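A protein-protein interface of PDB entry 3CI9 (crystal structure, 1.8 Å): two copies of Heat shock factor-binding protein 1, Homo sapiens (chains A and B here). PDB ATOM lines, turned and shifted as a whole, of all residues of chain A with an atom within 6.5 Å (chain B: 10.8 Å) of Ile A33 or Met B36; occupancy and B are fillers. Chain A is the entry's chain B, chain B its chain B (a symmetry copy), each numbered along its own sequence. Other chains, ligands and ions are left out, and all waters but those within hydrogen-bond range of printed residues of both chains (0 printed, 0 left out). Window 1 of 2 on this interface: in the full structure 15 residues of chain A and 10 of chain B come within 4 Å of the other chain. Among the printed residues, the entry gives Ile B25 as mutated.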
ATOM      1  N   GLN A  28     -28.422 -37.190  -9.113  1.00  0.00           N
ATOM      2  CA  GLN A  28     -27.589 -37.676 -10.189  1.00  0.00           C
ATOM      3  C   GLN A  28     -26.813 -36.506 -10.784  1.00  0.00           C
ATOM      4  O   GLN A  28     -25.624 -36.611 -11.077  1.00  0.00           O
ATOM      5  CB  GLN A  28     -28.493 -38.291 -11.238  1.00  0.00           C
ATOM      6  CG  GLN A  28     -27.818 -39.171 -12.244  1.00  0.00           C
ATOM      7  CD  GLN A  28     -28.771 -39.547 -13.358  1.00  0.00           C
ATOM      8  OE1 GLN A  28     -29.048 -38.736 -14.255  1.00  0.00           O
ATOM      9  NE2 GLN A  28     -29.304 -40.767 -13.295  1.00  0.00           N
ATOM     10  N   ILE A  29     -27.519 -35.394 -10.955  1.00  0.00           N
ATOM     11  CA  ILE A  29     -26.979 -34.163 -11.519  1.00  0.00           C
ATOM     12  C   ILE A  29     -25.972 -33.484 -10.597  1.00  0.00           C
ATOM     13  O   ILE A  29     -24.872 -33.137 -11.019  1.00  0.00           O
ATOM     14  CB  ILE A  29     -28.141 -33.180 -11.836  1.00  0.00           C
ATOM     15  CG1 ILE A  29     -28.917 -33.680 -13.065  1.00  0.00           C
ATOM     16  CG2 ILE A  29     -27.612 -31.767 -12.041  1.00  0.00           C
ATOM     17  CD1 ILE A  29     -30.155 -32.856 -13.418  1.00  0.00           C
ATOM     18  N   ILE A  30     -26.359 -33.289  -9.341  1.00  0.00           N
ATOM     19  CA  ILE A  30     -25.496 -32.645  -8.355  1.00  0.00           C
ATOM     20  C   ILE A  30     -24.173 -33.401  -8.209  1.00  0.00           C
ATOM     21  O   ILE A  30     -23.121 -32.798  -7.984  1.00  0.00           O
ATOM     22  CB  ILE A  30     -26.205 -32.558  -6.969  1.00  0.00           C
ATOM     23  CG1 ILE A  30     -27.495 -31.736  -7.093  1.00  0.00           C
ATOM     24  CG2 ILE A  30     -25.277 -31.925  -5.939  1.00  0.00           C
ATOM     25  CD1 ILE A  30     -28.255 -31.556  -5.797  1.00  0.00           C
ATOM     26  N   GLY A  31     -24.237 -34.723  -8.338  1.00  0.00           N
ATOM     27  CA  GLY A  31     -23.038 -35.529  -8.239  1.00  0.00           C
ATOM     28  C   GLY A  31     -22.102 -35.186  -9.377  1.00  0.00           C
ATOM     29  O   GLY A  31     -20.902 -35.075  -9.173  1.00  0.00           O
ATOM     30  N   ARG A  32     -22.651 -35.012 -10.579  1.00  0.00           N
ATOM     31  CA  ARG A  32     -21.848 -34.675 -11.758  1.00  0.00           C
ATOM     32  C   ARG A  32     -21.212 -33.289 -11.625  1.00  0.00           C
ATOM     33  O   ARG A  32     -20.042 -33.100 -11.949  1.00  0.00           O
ATOM     34  CB  ARG A  32     -22.704 -34.733 -13.029  1.00  0.00           C
ATOM     35  CG  ARG A  32     -23.155 -36.139 -13.421  1.00  0.00           C
ATOM     36  CD  ARG A  32     -23.847 -36.147 -14.776  1.00  0.00           C
ATOM     37  NE  ARG A  32     -22.913 -35.834 -15.854  1.00  0.00           N
ATOM     38  CZ  ARG A  32     -23.267 -35.577 -17.110  1.00  0.00           C
ATOM     39  NH1 ARG A  32     -24.542 -35.589 -17.466  1.00  0.00           N
ATOM     40  NH2 ARG A  32     -22.340 -35.295 -18.017  1.00  0.00           N
ATOM     41  N   ILE A  33     -21.992 -32.329 -11.141  1.00  0.00           N
ATOM     42  CA  ILE A  33     -21.512 -30.968 -10.935  1.00  0.00           C
ATOM     43  C   ILE A  33     -20.417 -30.980  -9.882  1.00  0.00           C
ATOM     44  O   ILE A  33     -19.419 -30.280  -9.989  1.00  0.00           O
ATOM     45  CB  ILE A  33     -22.651 -30.062 -10.444  1.00  0.00           C
ATOM     46  CG1 ILE A  33     -23.820 -30.133 -11.429  1.00  0.00           C
ATOM     47  CG2 ILE A  33     -22.164 -28.633 -10.311  1.00  0.00           C
ATOM     48  CD1 ILE A  33     -25.047 -29.414 -10.961  1.00  0.00           C
ATOM     49  N   ASP A  34     -20.607 -31.788  -8.850  1.00  0.00           N
ATOM     50  CA  ASP A  34     -19.611 -31.859  -7.796  1.00  0.00           C
ATOM     51  C   ASP A  34     -18.286 -32.374  -8.325  1.00  0.00           C
ATOM     52  O   ASP A  34     -17.230 -31.926  -7.890  1.00  0.00           O
ATOM     53  CB  ASP A  34     -20.102 -32.747  -6.645  1.00  0.00           C
ATOM     54  CG  ASP A  34     -21.224 -32.093  -5.847  1.00  0.00           C
ATOM     55  OD1 ASP A  34     -21.094 -30.895  -5.528  1.00  0.00           O
ATOM     56  OD2 ASP A  34     -22.227 -32.769  -5.533  1.00  0.00           O
ATOM     57  N   ASP A  35     -18.331 -33.310  -9.269  1.00  0.00           N
ATOM     58  CA  ASP A  35     -17.093 -33.839  -9.818  1.00  0.00           C
ATOM     59  C   ASP A  35     -16.480 -32.835 -10.784  1.00  0.00           C
ATOM     60  O   ASP A  35     -15.253 -32.725 -10.877  1.00  0.00           O
ATOM     61  CB  ASP A  35     -17.333 -35.156 -10.542  1.00  0.00           C
ATOM     62  CG  ASP A  35     -16.043 -35.861 -10.886  1.00  0.00           C
ATOM     63  OD1 ASP A  35     -16.085 -36.825 -11.677  1.00  0.00           O
ATOM     64  OD2 ASP A  35     -14.983 -35.454 -10.360  1.00  0.00           O
ATOM     65  N   MET A  36     -17.341 -32.110 -11.502  1.00  0.00           N
ATOM     66  CA  MET A  36     -16.901 -31.081 -12.448  1.00  0.00           C
ATOM     67  C   MET A  36     -16.231 -29.935 -11.688  1.00  0.00           C
ATOM     68  O   MET A  36     -15.198 -29.416 -12.106  1.00  0.00           O
ATOM     69  CB  MET A  36     -18.091 -30.523 -13.233  1.00  0.00           C
ATOM     70  CG  MET A  36     -18.749 -31.496 -14.191  1.00  0.00           C
ATOM     71  SD  MET A  36     -20.166 -30.747 -15.011  1.00  0.00           S
ATOM     72  CE  MET A  36     -19.371 -29.556 -16.107  1.00  0.00           C
ATOM     73  N   SER A  37     -16.825 -29.531 -10.570  1.00  0.00           N
ATOM     74  CA  SER A  37     -16.240 -28.457  -9.779  1.00  0.00           C
ATOM     75  C   SER A  37     -14.854 -28.892  -9.331  1.00  0.00           C
ATOM     76  O   SER A  37     -13.912 -28.097  -9.324  1.00  0.00           O
ATOM     77  CB  SER A  37     -17.108 -28.171  -8.565  1.00  0.00           C
ATOM     78  OG  SER A  37     -18.419 -27.845  -8.980  1.00  0.00           O
ATOM     79  N   SER A  38     -14.739 -30.165  -8.967  1.00  0.00           N
ATOM     80  CA  SER A  38     -13.476 -30.727  -8.520  1.00  0.00           C
ATOM     81  C   SER A  38     -12.407 -30.522  -9.586  1.00  0.00           C
ATOM     82  O   SER A  38     -11.308 -30.045  -9.299  1.00  0.00           O
ATOM     83  CB  SER A  38     -13.637 -32.218  -8.235  1.00  0.00           C
ATOM     84  OG  SER A  38     -12.455 -32.750  -7.665  1.00  0.00           O
ATOM     85  N   ILE A  40     -12.506 -28.421 -12.175  1.00  0.00           N
ATOM     86  CA  ILE A  40     -12.262 -27.005 -12.411  1.00  0.00           C
ATOM     87  C   ILE A  40     -11.295 -26.455 -11.359  1.00  0.00           C
ATOM     88  O   ILE A  40     -10.405 -25.663 -11.677  1.00  0.00           O
ATOM     89  CB  ILE A  40     -13.554 -26.187 -12.363  1.00  0.00           C
ATOM     90  CG1 ILE A  40     -14.566 -26.735 -13.376  1.00  0.00           C
ATOM     91  CG2 ILE A  40     -13.233 -24.722 -12.656  1.00  0.00           C
ATOM     92  CD1 ILE A  40     -15.942 -26.075 -13.321  1.00  0.00           C
ATOM     93  N   ILE B  25     -34.461 -26.678  -5.794  1.00  0.00           N
ATOM     94  CA  ILE B  25     -33.278 -27.469  -6.097  1.00  0.00           C
ATOM     95  C   ILE B  25     -32.745 -27.074  -7.471  1.00  0.00           C
ATOM     96  O   ILE B  25     -31.541 -26.947  -7.663  1.00  0.00           O
ATOM     97  CB  ILE B  25     -33.599 -28.991  -6.079  1.00  0.00           C
ATOM     98  CG1 ILE B  25     -34.082 -29.400  -4.681  1.00  0.00           C
ATOM     99  CG2 ILE B  25     -32.360 -29.804  -6.485  1.00  0.00           C
ATOM    100  CD1 ILE B  25     -34.377 -30.885  -4.526  1.00  0.00           C
ATOM    101  N   SER B  26     -33.645 -26.868  -8.420  1.00  0.00           N
ATOM    102  CA  SER B  26     -33.241 -26.497  -9.764  1.00  0.00           C
ATOM    103  C   SER B  26     -32.507 -25.165  -9.770  1.00  0.00           C
ATOM    104  O   SER B  26     -31.346 -25.097 -10.171  1.00  0.00           O
ATOM    105  CB  SER B  26     -34.461 -26.416 -10.677  1.00  0.00           C
ATOM    106  OG  SER B  26     -35.148 -27.654 -10.703  1.00  0.00           O
ATOM    107  N   ASP B  27     -33.187 -24.106  -9.335  1.00  0.00           N
ATOM    108  CA  ASP B  27     -32.591 -22.774  -9.290  1.00  0.00           C
ATOM    109  C   ASP B  27     -31.244 -22.824  -8.577  1.00  0.00           C
ATOM    110  O   ASP B  27     -30.318 -22.074  -8.886  1.00  0.00           O
ATOM    111  CB  ASP B  27     -33.527 -21.797  -8.562  1.00  0.00           C
ATOM    112  CG  ASP B  27     -34.756 -21.437  -9.387  1.00  0.00           C
ATOM    113  OD1 ASP B  27     -34.586 -21.014 -10.547  1.00  0.00           O
ATOM    114  OD2 ASP B  27     -35.895 -21.566  -8.882  1.00  0.00           O
ATOM    115  N   GLN B  28     -31.146 -23.735  -7.624  1.00  0.00           N
ATOM    116  CA  GLN B  28     -29.943 -23.912  -6.843  1.00  0.00           C
ATOM    117  C   GLN B  28     -28.845 -24.469  -7.742  1.00  0.00           C
ATOM    118  O   GLN B  28     -27.693 -24.043  -7.681  1.00  0.00           O
ATOM    119  CB  GLN B  28     -30.251 -24.890  -5.727  1.00  0.00           C
ATOM    120  CG  GLN B  28     -29.264 -24.925  -4.603  1.00  0.00           C
ATOM    121  CD  GLN B  28     -29.553 -26.079  -3.667  1.00  0.00           C
ATOM    122  OE1 GLN B  28     -29.239 -27.240  -3.975  1.00  0.00           O
ATOM    123  NE2 GLN B  28     -30.180 -25.777  -2.529  1.00  0.00           N
ATOM    124  N   ILE B  29     -29.232 -25.430  -8.572  1.00  0.00           N
ATOM    125  CA  ILE B  29     -28.344 -26.108  -9.508  1.00  0.00           C
ATOM    126  C   ILE B  29     -27.876 -25.201 -10.639  1.00  0.00           C
ATOM    127  O   ILE B  29     -26.683 -25.111 -10.919  1.00  0.00           O
ATOM    128  CB  ILE B  29     -29.062 -27.354 -10.100  1.00  0.00           C
ATOM    129  CG1 ILE B  29     -29.155 -28.452  -9.028  1.00  0.00           C
ATOM    130  CG2 ILE B  29     -28.344 -27.847 -11.349  1.00  0.00           C
ATOM    131  CD1 ILE B  29     -29.938 -29.694  -9.452  1.00  0.00           C
ATOM    132  N   ILE B  30     -28.824 -24.540 -11.296  1.00  0.00           N
ATOM    133  CA  ILE B  30     -28.515 -23.641 -12.405  1.00  0.00           C
ATOM    134  C   ILE B  30     -27.548 -22.540 -11.967  1.00  0.00           C
ATOM    135  O   ILE B  30     -26.695 -22.100 -12.741  1.00  0.00           O
ATOM    136  CB  ILE B  30     -29.816 -22.998 -12.977  1.00  0.00           C
ATOM    137  CG1 ILE B  30     -30.758 -24.095 -13.490  1.00  0.00           C
ATOM    138  CG2 ILE B  30     -29.476 -22.030 -14.104  1.00  0.00           C
ATOM    139  CD1 ILE B  30     -32.046 -23.585 -14.099  1.00  0.00           C
ATOM    140  N   GLY B  31     -27.687 -22.102 -10.719  1.00  0.00           N
ATOM    141  CA  GLY B  31     -26.807 -21.077 -10.198  1.00  0.00           C
ATOM    142  C   GLY B  31     -25.390 -21.604 -10.146  1.00  0.00           C
ATOM    143  O   GLY B  31     -24.457 -20.893 -10.493  1.00  0.00           O
ATOM    144  N   ARG B  32     -25.227 -22.855  -9.720  1.00  0.00           N
ATOM    145  CA  ARG B  32     -23.903 -23.479  -9.628  1.00  0.00           C
ATOM    146  C   ARG B  32     -23.270 -23.654 -11.011  1.00  0.00           C
ATOM    147  O   ARG B  32     -22.086 -23.387 -11.198  1.00  0.00           O
ATOM    148  CB  ARG B  32     -23.993 -24.839  -8.925  1.00  0.00           C
ATOM    149  CG  ARG B  32     -24.340 -24.757  -7.439  1.00  0.00           C
ATOM    150  CD  ARG B  32     -24.241 -26.117  -6.765  1.00  0.00           C
ATOM    151  NE  ARG B  32     -22.860 -26.588  -6.712  1.00  0.00           N
ATOM    152  CZ  ARG B  32     -22.493 -27.817  -6.364  1.00  0.00           C
ATOM    153  NH1 ARG B  32     -23.402 -28.723  -6.033  1.00  0.00           N
ATOM    154  NH2 ARG B  32     -21.208 -28.150  -6.355  1.00  0.00           N
ATOM    155  N   ILE B  33     -24.072 -24.096 -11.973  1.00  0.00           N
ATOM    156  CA  ILE B  33     -23.611 -24.284 -13.343  1.00  0.00           C
ATOM    157  C   ILE B  33     -23.215 -22.939 -13.925  1.00  0.00           C
ATOM    158  O   ILE B  33     -22.229 -22.816 -14.638  1.00  0.00           O
ATOM    159  CB  ILE B  33     -24.730 -24.880 -14.212  1.00  0.00           C
ATOM    160  CG1 ILE B  33     -25.234 -26.177 -13.576  1.00  0.00           C
ATOM    161  CG2 ILE B  33     -24.219 -25.148 -15.613  1.00  0.00           C
ATOM    162  CD1 ILE B  33     -26.436 -26.754 -14.255  1.00  0.00           C
ATOM    163  N   ASP B  34     -23.994 -21.914 -13.613  1.00  0.00           N
ATOM    164  CA  ASP B  34     -23.689 -20.592 -14.128  1.00  0.00           C
ATOM    165  C   ASP B  34     -22.348 -20.099 -13.618  1.00  0.00           C
ATOM    166  O   ASP B  34     -21.618 -19.432 -14.344  1.00  0.00           O
ATOM    167  CB  ASP B  34     -24.795 -19.596 -13.756  1.00  0.00           C
ATOM    168  CG  ASP B  34     -26.084 -19.845 -14.530  1.00  0.00           C
ATOM    169  OD1 ASP B  34     -25.998 -20.055 -15.756  1.00  0.00           O
ATOM    170  OD2 ASP B  34     -27.177 -19.826 -13.925  1.00  0.00           O
ATOM    171  N   ASP B  35     -22.014 -20.427 -12.374  1.00  0.00           N
ATOM    172  CA  ASP B  35     -20.738 -19.986 -11.832  1.00  0.00           C
ATOM    173  C   ASP B  35     -19.608 -20.832 -12.402  1.00  0.00           C
ATOM    174  O   ASP B  35     -18.502 -20.330 -12.624  1.00  0.00           O
ATOM    175  CB  ASP B  35     -20.725 -20.083 -10.312  1.00  0.00           C
ATOM    176  CG  ASP B  35     -19.530 -19.388  -9.706  1.00  0.00           C
ATOM    177  OD1 ASP B  35     -19.273 -19.589  -8.502  1.00  0.00           O
ATOM    178  OD2 ASP B  35     -18.847 -18.635 -10.434  1.00  0.00           O
ATOM    179  N   MET B  36     -19.895 -22.115 -12.634  1.00  0.00           N
ATOM    180  CA  MET B  36     -18.920 -23.043 -13.213  1.00  0.00           C
ATOM    181  C   MET B  36     -18.604 -22.628 -14.651  1.00  0.00           C
ATOM    182  O   MET B  36     -17.451 -22.643 -15.076  1.00  0.00           O
ATOM    183  CB  MET B  36     -19.472 -24.471 -13.222  1.00  0.00           C
ATOM    184  CG  MET B  36     -19.657 -25.103 -11.856  1.00  0.00           C
ATOM    185  SD  MET B  36     -20.363 -26.755 -11.992  1.00  0.00           S
ATOM    186  CE  MET B  36     -18.991 -27.686 -12.701  1.00  0.00           C
ATOM    187  N   SER B  37     -19.633 -22.264 -15.408  1.00  0.00           N
ATOM    188  CA  SER B  37     -19.415 -21.837 -16.783  1.00  0.00           C
ATOM    189  C   SER B  37     -18.510 -20.615 -16.767  1.00  0.00           C
ATOM    190  O   SER B  37     -17.619 -20.477 -17.608  1.00  0.00           O
ATOM    191  CB  SER B  37     -20.740 -21.488 -17.439  1.00  0.00           C
ATOM    192  OG  SER B  37     -21.610 -22.600 -17.381  1.00  0.00           O
ATOM    193  N   SER B  38     -18.743 -19.738 -15.796  1.00  0.00           N
ATOM    194  CA  SER B  38     -17.957 -18.525 -15.650  1.00  0.00           C
ATOM    195  C   SER B  38     -16.479 -18.872 -15.524  1.00  0.00           C
ATOM    196  O   SER B  38     -15.633 -18.307 -16.219  1.00  0.00           O
ATOM    197  CB  SER B  38     -18.410 -17.752 -14.413  1.00  0.00           C
ATOM    198  OG  SER B  38     -17.752 -16.502 -14.335  1.00  0.00           O
ATOM    199  N   ARG B  39     -16.178 -19.804 -14.627  1.00  0.00           N
ATOM    200  CA  ARG B  39     -14.807 -20.239 -14.399  1.00  0.00           C
ATOM    201  C   ARG B  39     -14.226 -20.906 -15.646  1.00  0.00           C
ATOM    202  O   ARG B  39     -13.081 -20.653 -16.020  1.00  0.00           O
ATOM    203  CB  ARG B  39     -14.767 -21.210 -13.222  1.00  0.00           C
ATOM    204  CG  ARG B  39     -15.429 -20.673 -11.973  1.00  0.00           C
ATOM    205  CD  ARG B  39     -15.592 -21.754 -10.898  1.00  0.00           C
ATOM    206  NE  ARG B  39     -14.317 -22.214 -10.351  1.00  0.00           N
ATOM    207  CZ  ARG B  39     -14.200 -23.179  -9.440  1.00  0.00           C
ATOM    208  NH1 ARG B  39     -15.284 -23.793  -8.975  1.00  0.00           N
ATOM    209  NH2 ARG B  39     -13.003 -23.533  -8.986  1.00  0.00           N
ATOM    210  N   ILE B  40     -15.006 -21.764 -16.296  1.00  0.00           N
ATOM    211  CA  ILE B  40     -14.515 -22.425 -17.496  1.00  0.00           C
ATOM    212  C   ILE B  40     -14.162 -21.386 -18.563  1.00  0.00           C
ATOM    213  O   ILE B  40     -13.151 -21.514 -19.256  1.00  0.00           O
ATOM    214  CB  ILE B  40     -15.549 -23.393 -18.078  1.00  0.00           C
ATOM    215  CG1 ILE B  40     -15.959 -24.426 -17.023  1.00  0.00           C
ATOM    216  CG2 ILE B  40     -14.957 -24.079 -19.309  1.00  0.00           C
ATOM    217  CD1 ILE B  40     -17.085 -25.363 -17.455  1.00  0.00           C
ATOM    218  N   ASP B  41     -15.002 -20.362 -18.700  1.00  0.00           N
ATOM    219  CA  ASP B  41     -14.740 -19.311 -19.675  1.00  0.00           C
ATOM    220  C   ASP B  41     -13.348 -18.729 -19.421  1.00  0.00           C
ATOM    221  O   ASP B  41     -12.529 -18.611 -20.331  1.00  0.00           O
ATOM    222  CB  ASP B  41     -15.772 -18.180 -19.561  1.00  0.00           C
ATOM    223  CG  ASP B  41     -17.132 -18.543 -20.146  1.00  0.00           C
ATOM    224  OD1 ASP B  41     -17.235 -19.519 -20.916  1.00  0.00           O
ATOM    225  OD2 ASP B  41     -18.105 -17.817 -19.842  1.00  0.00           O
ATOM    226  N   ASP B  42     -13.088 -18.370 -18.170  1.00  0.00           N
ATOM    227  CA  ASP B  42     -11.814 -17.782 -17.789  1.00  0.00           C
ATOM    228  C   ASP B  42     -10.633 -18.726 -17.997  1.00  0.00           C
ATOM    229  O   ASP B  42      -9.544 -18.292 -18.382  1.00  0.00           O
ATOM    230  CB  ASP B  42     -11.874 -17.312 -16.333  1.00  0.00           C
ATOM    231  CG  ASP B  42     -12.799 -16.127 -16.148  1.00  0.00           C
ATOM    232  OD1 ASP B  42     -12.979 -15.687 -14.991  1.00  0.00           O
ATOM    233  OD2 ASP B  42     -13.345 -15.636 -17.163  1.00  0.00           O
ATOM    234  N   LEU B  43     -10.845 -20.011 -17.727  1.00  0.00           N
ATOM    235  CA  LEU B  43      -9.794 -21.001 -17.918  1.00  0.00           C
ATOM    236  C   LEU B  43      -9.434 -21.069 -19.401  1.00  0.00           C
ATOM    237  O   LEU B  43      -8.259 -21.065 -19.757  1.00  0.00           O
ATOM    238  CB  LEU B  43     -10.256 -22.382 -17.438  1.00  0.00           C
ATOM    239  CG  LEU B  43     -10.160 -22.655 -15.935  1.00  0.00           C
ATOM    240  CD1 LEU B  43     -10.885 -23.953 -15.585  1.00  0.00           C
ATOM    241  CD2 LEU B  43      -8.683 -22.721 -15.538  1.00  0.00           C
ATOM    242  N   GLU B  44     -10.447 -21.127 -20.263  1.00  0.00           N
ATOM    243  CA  GLU B  44     -10.207 -21.202 -21.701  1.00  0.00           C
ATOM    244  C   GLU B  44      -9.556 -19.929 -22.195  1.00  0.00           C
ATOM    245  O   GLU B  44      -8.729 -19.965 -23.102  1.00  0.00           O
ATOM    246  CB  GLU B  44     -11.511 -21.409 -22.458  1.00  0.00           C
ATOM    247  CG  GLU B  44     -12.319 -22.584 -21.962  1.00  0.00           C
ATOM    248  CD  GLU B  44     -13.633 -22.726 -22.703  1.00  0.00           C
ATOM    249  OE1 GLU B  44     -14.291 -21.686 -22.944  1.00  0.00           O
ATOM    250  OE2 GLU B  44     -14.005 -23.877 -23.035  1.00  0.00           O
ATOM    251  N   LYS B  45      -9.945 -18.804 -21.596  1.00  0.00           N
ATOM    252  CA  LYS B  45      -9.391 -17.508 -21.969  1.00  0.00           C
ATOM    253  C   LYS B  45      -7.921 -17.412 -21.599  1.00  0.00           C
ATOM    254  O   LYS B  45      -7.106 -16.915 -22.375  1.00  0.00           O
ATOM    255  CB  LYS B  45     -10.150 -16.382 -21.275  1.00  0.00           C
ATOM    256  CG  LYS B  45     -11.571 -16.163 -21.767  1.00  0.00           C
ATOM    257  CD  LYS B  45     -12.154 -14.962 -21.064  1.00  0.00           C
ATOM    258  CE  LYS B  45     -13.476 -14.557 -21.647  1.00  0.00           C
ATOM    259  NZ  LYS B  45     -13.792 -13.167 -21.223  1.00  0.00           N
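Ile A33 touches two residues of chain B.
No residue of chain B comes within 4 Å of Ile A29.
Of chain B, only Ile B29 (3.96 Å) and Arg B32 (3.7 Å) come within 4 Å of Ile A30.
No residue of chain B comes within 4 Å of Gly A31.
Printed residues of chain B within 4 Å of Asp A34: Arg B32.
Met A36 touches just one residue of chain B: Met B36 (3.0 Å).
Of chain B, only Arg B32 and Met B36 come within 4 Å of Ser A37.
Of the printed residues of chain A, Ile B29 touches Ile A30 and Ile A33.
Of the printed residues of chain A, Leu B43 touches Ile A40 (3.8 Å).
The nearest residue of chain B that does not touch Ile A33 is Arg B32 (4.04 Å).
The nearest printed residue of chain A that does not touch Ile B29 is Ile A29 (4.05 Å).
The side-chain hydroxyl (OG) of Ser A37 is in hydrogen-bond range of the side-chain sulfur (SD) of Met B36 (3.7 Å).
The guanidinium group of Arg B32 lies within salt-bridge range of the side-chain carboxylate of Asp A34, 2.9 Å away.
The backbone carbonyl oxygen of Ile A33 is in hydrogen-bond range of the side-chain hydroxyl of Ser A37 (2.8 Å).
The side-chain carboxylate (OD2) of Asp A34 lies close to the backbone carbonyl oxygen (O) of Ile A30 (2.6 Å).
Among the printed residues, pairs that only touch across the chains: Met A36 with Met B36 (3.0 Å), Ile A33 with Met B36 (3.1 Å), Ile A40 with Met B36 (3.5 Å), Ile A40 with Arg B39 (3.6 Å), Ile A33 with Ile B29 (3.7 Å), Ile A30 with Arg B32 (3.7 Å), Ile A40 with Leu B43 (3.8 Å), Ser A37 with Arg B32 (3.8 Å) and Ile A30 with Ile B29 (3.96 Å).
Hydrophobic or aromatic side chains of chain A that line the printed part of chain B: Ile A30, Ile A33, Met A36 and Ile A40.
Of the 21 printed residues of chain B, 5 touch a printed residue of chain A.
Among the printed residues, Asp or Glu carboxylates within 4 Å of a Lys or Arg side-chain nitrogen of the other chain: Asp A34 with Arg B32 (2.9 Å).
Ile A30 touches Ile B29, but with the chains exchanged Ile A29 does not touch Ile B30 (7.4 Å).
Met A36 touches its own counterpart, Met B36.
Ser A37 touches Met B36, but with the chains exchanged Met A36 does not touch Ser B37 (7.3 Å).
Ile A40 touches Met B36, but with the chains exchanged Met A36 does not touch Ile B40 (5.0 Å).
12 positions are printed for both chains.
Of the 11 pairs that touch across the chains among the printed residues, 1 has its exchanged pair printed and touching as well.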
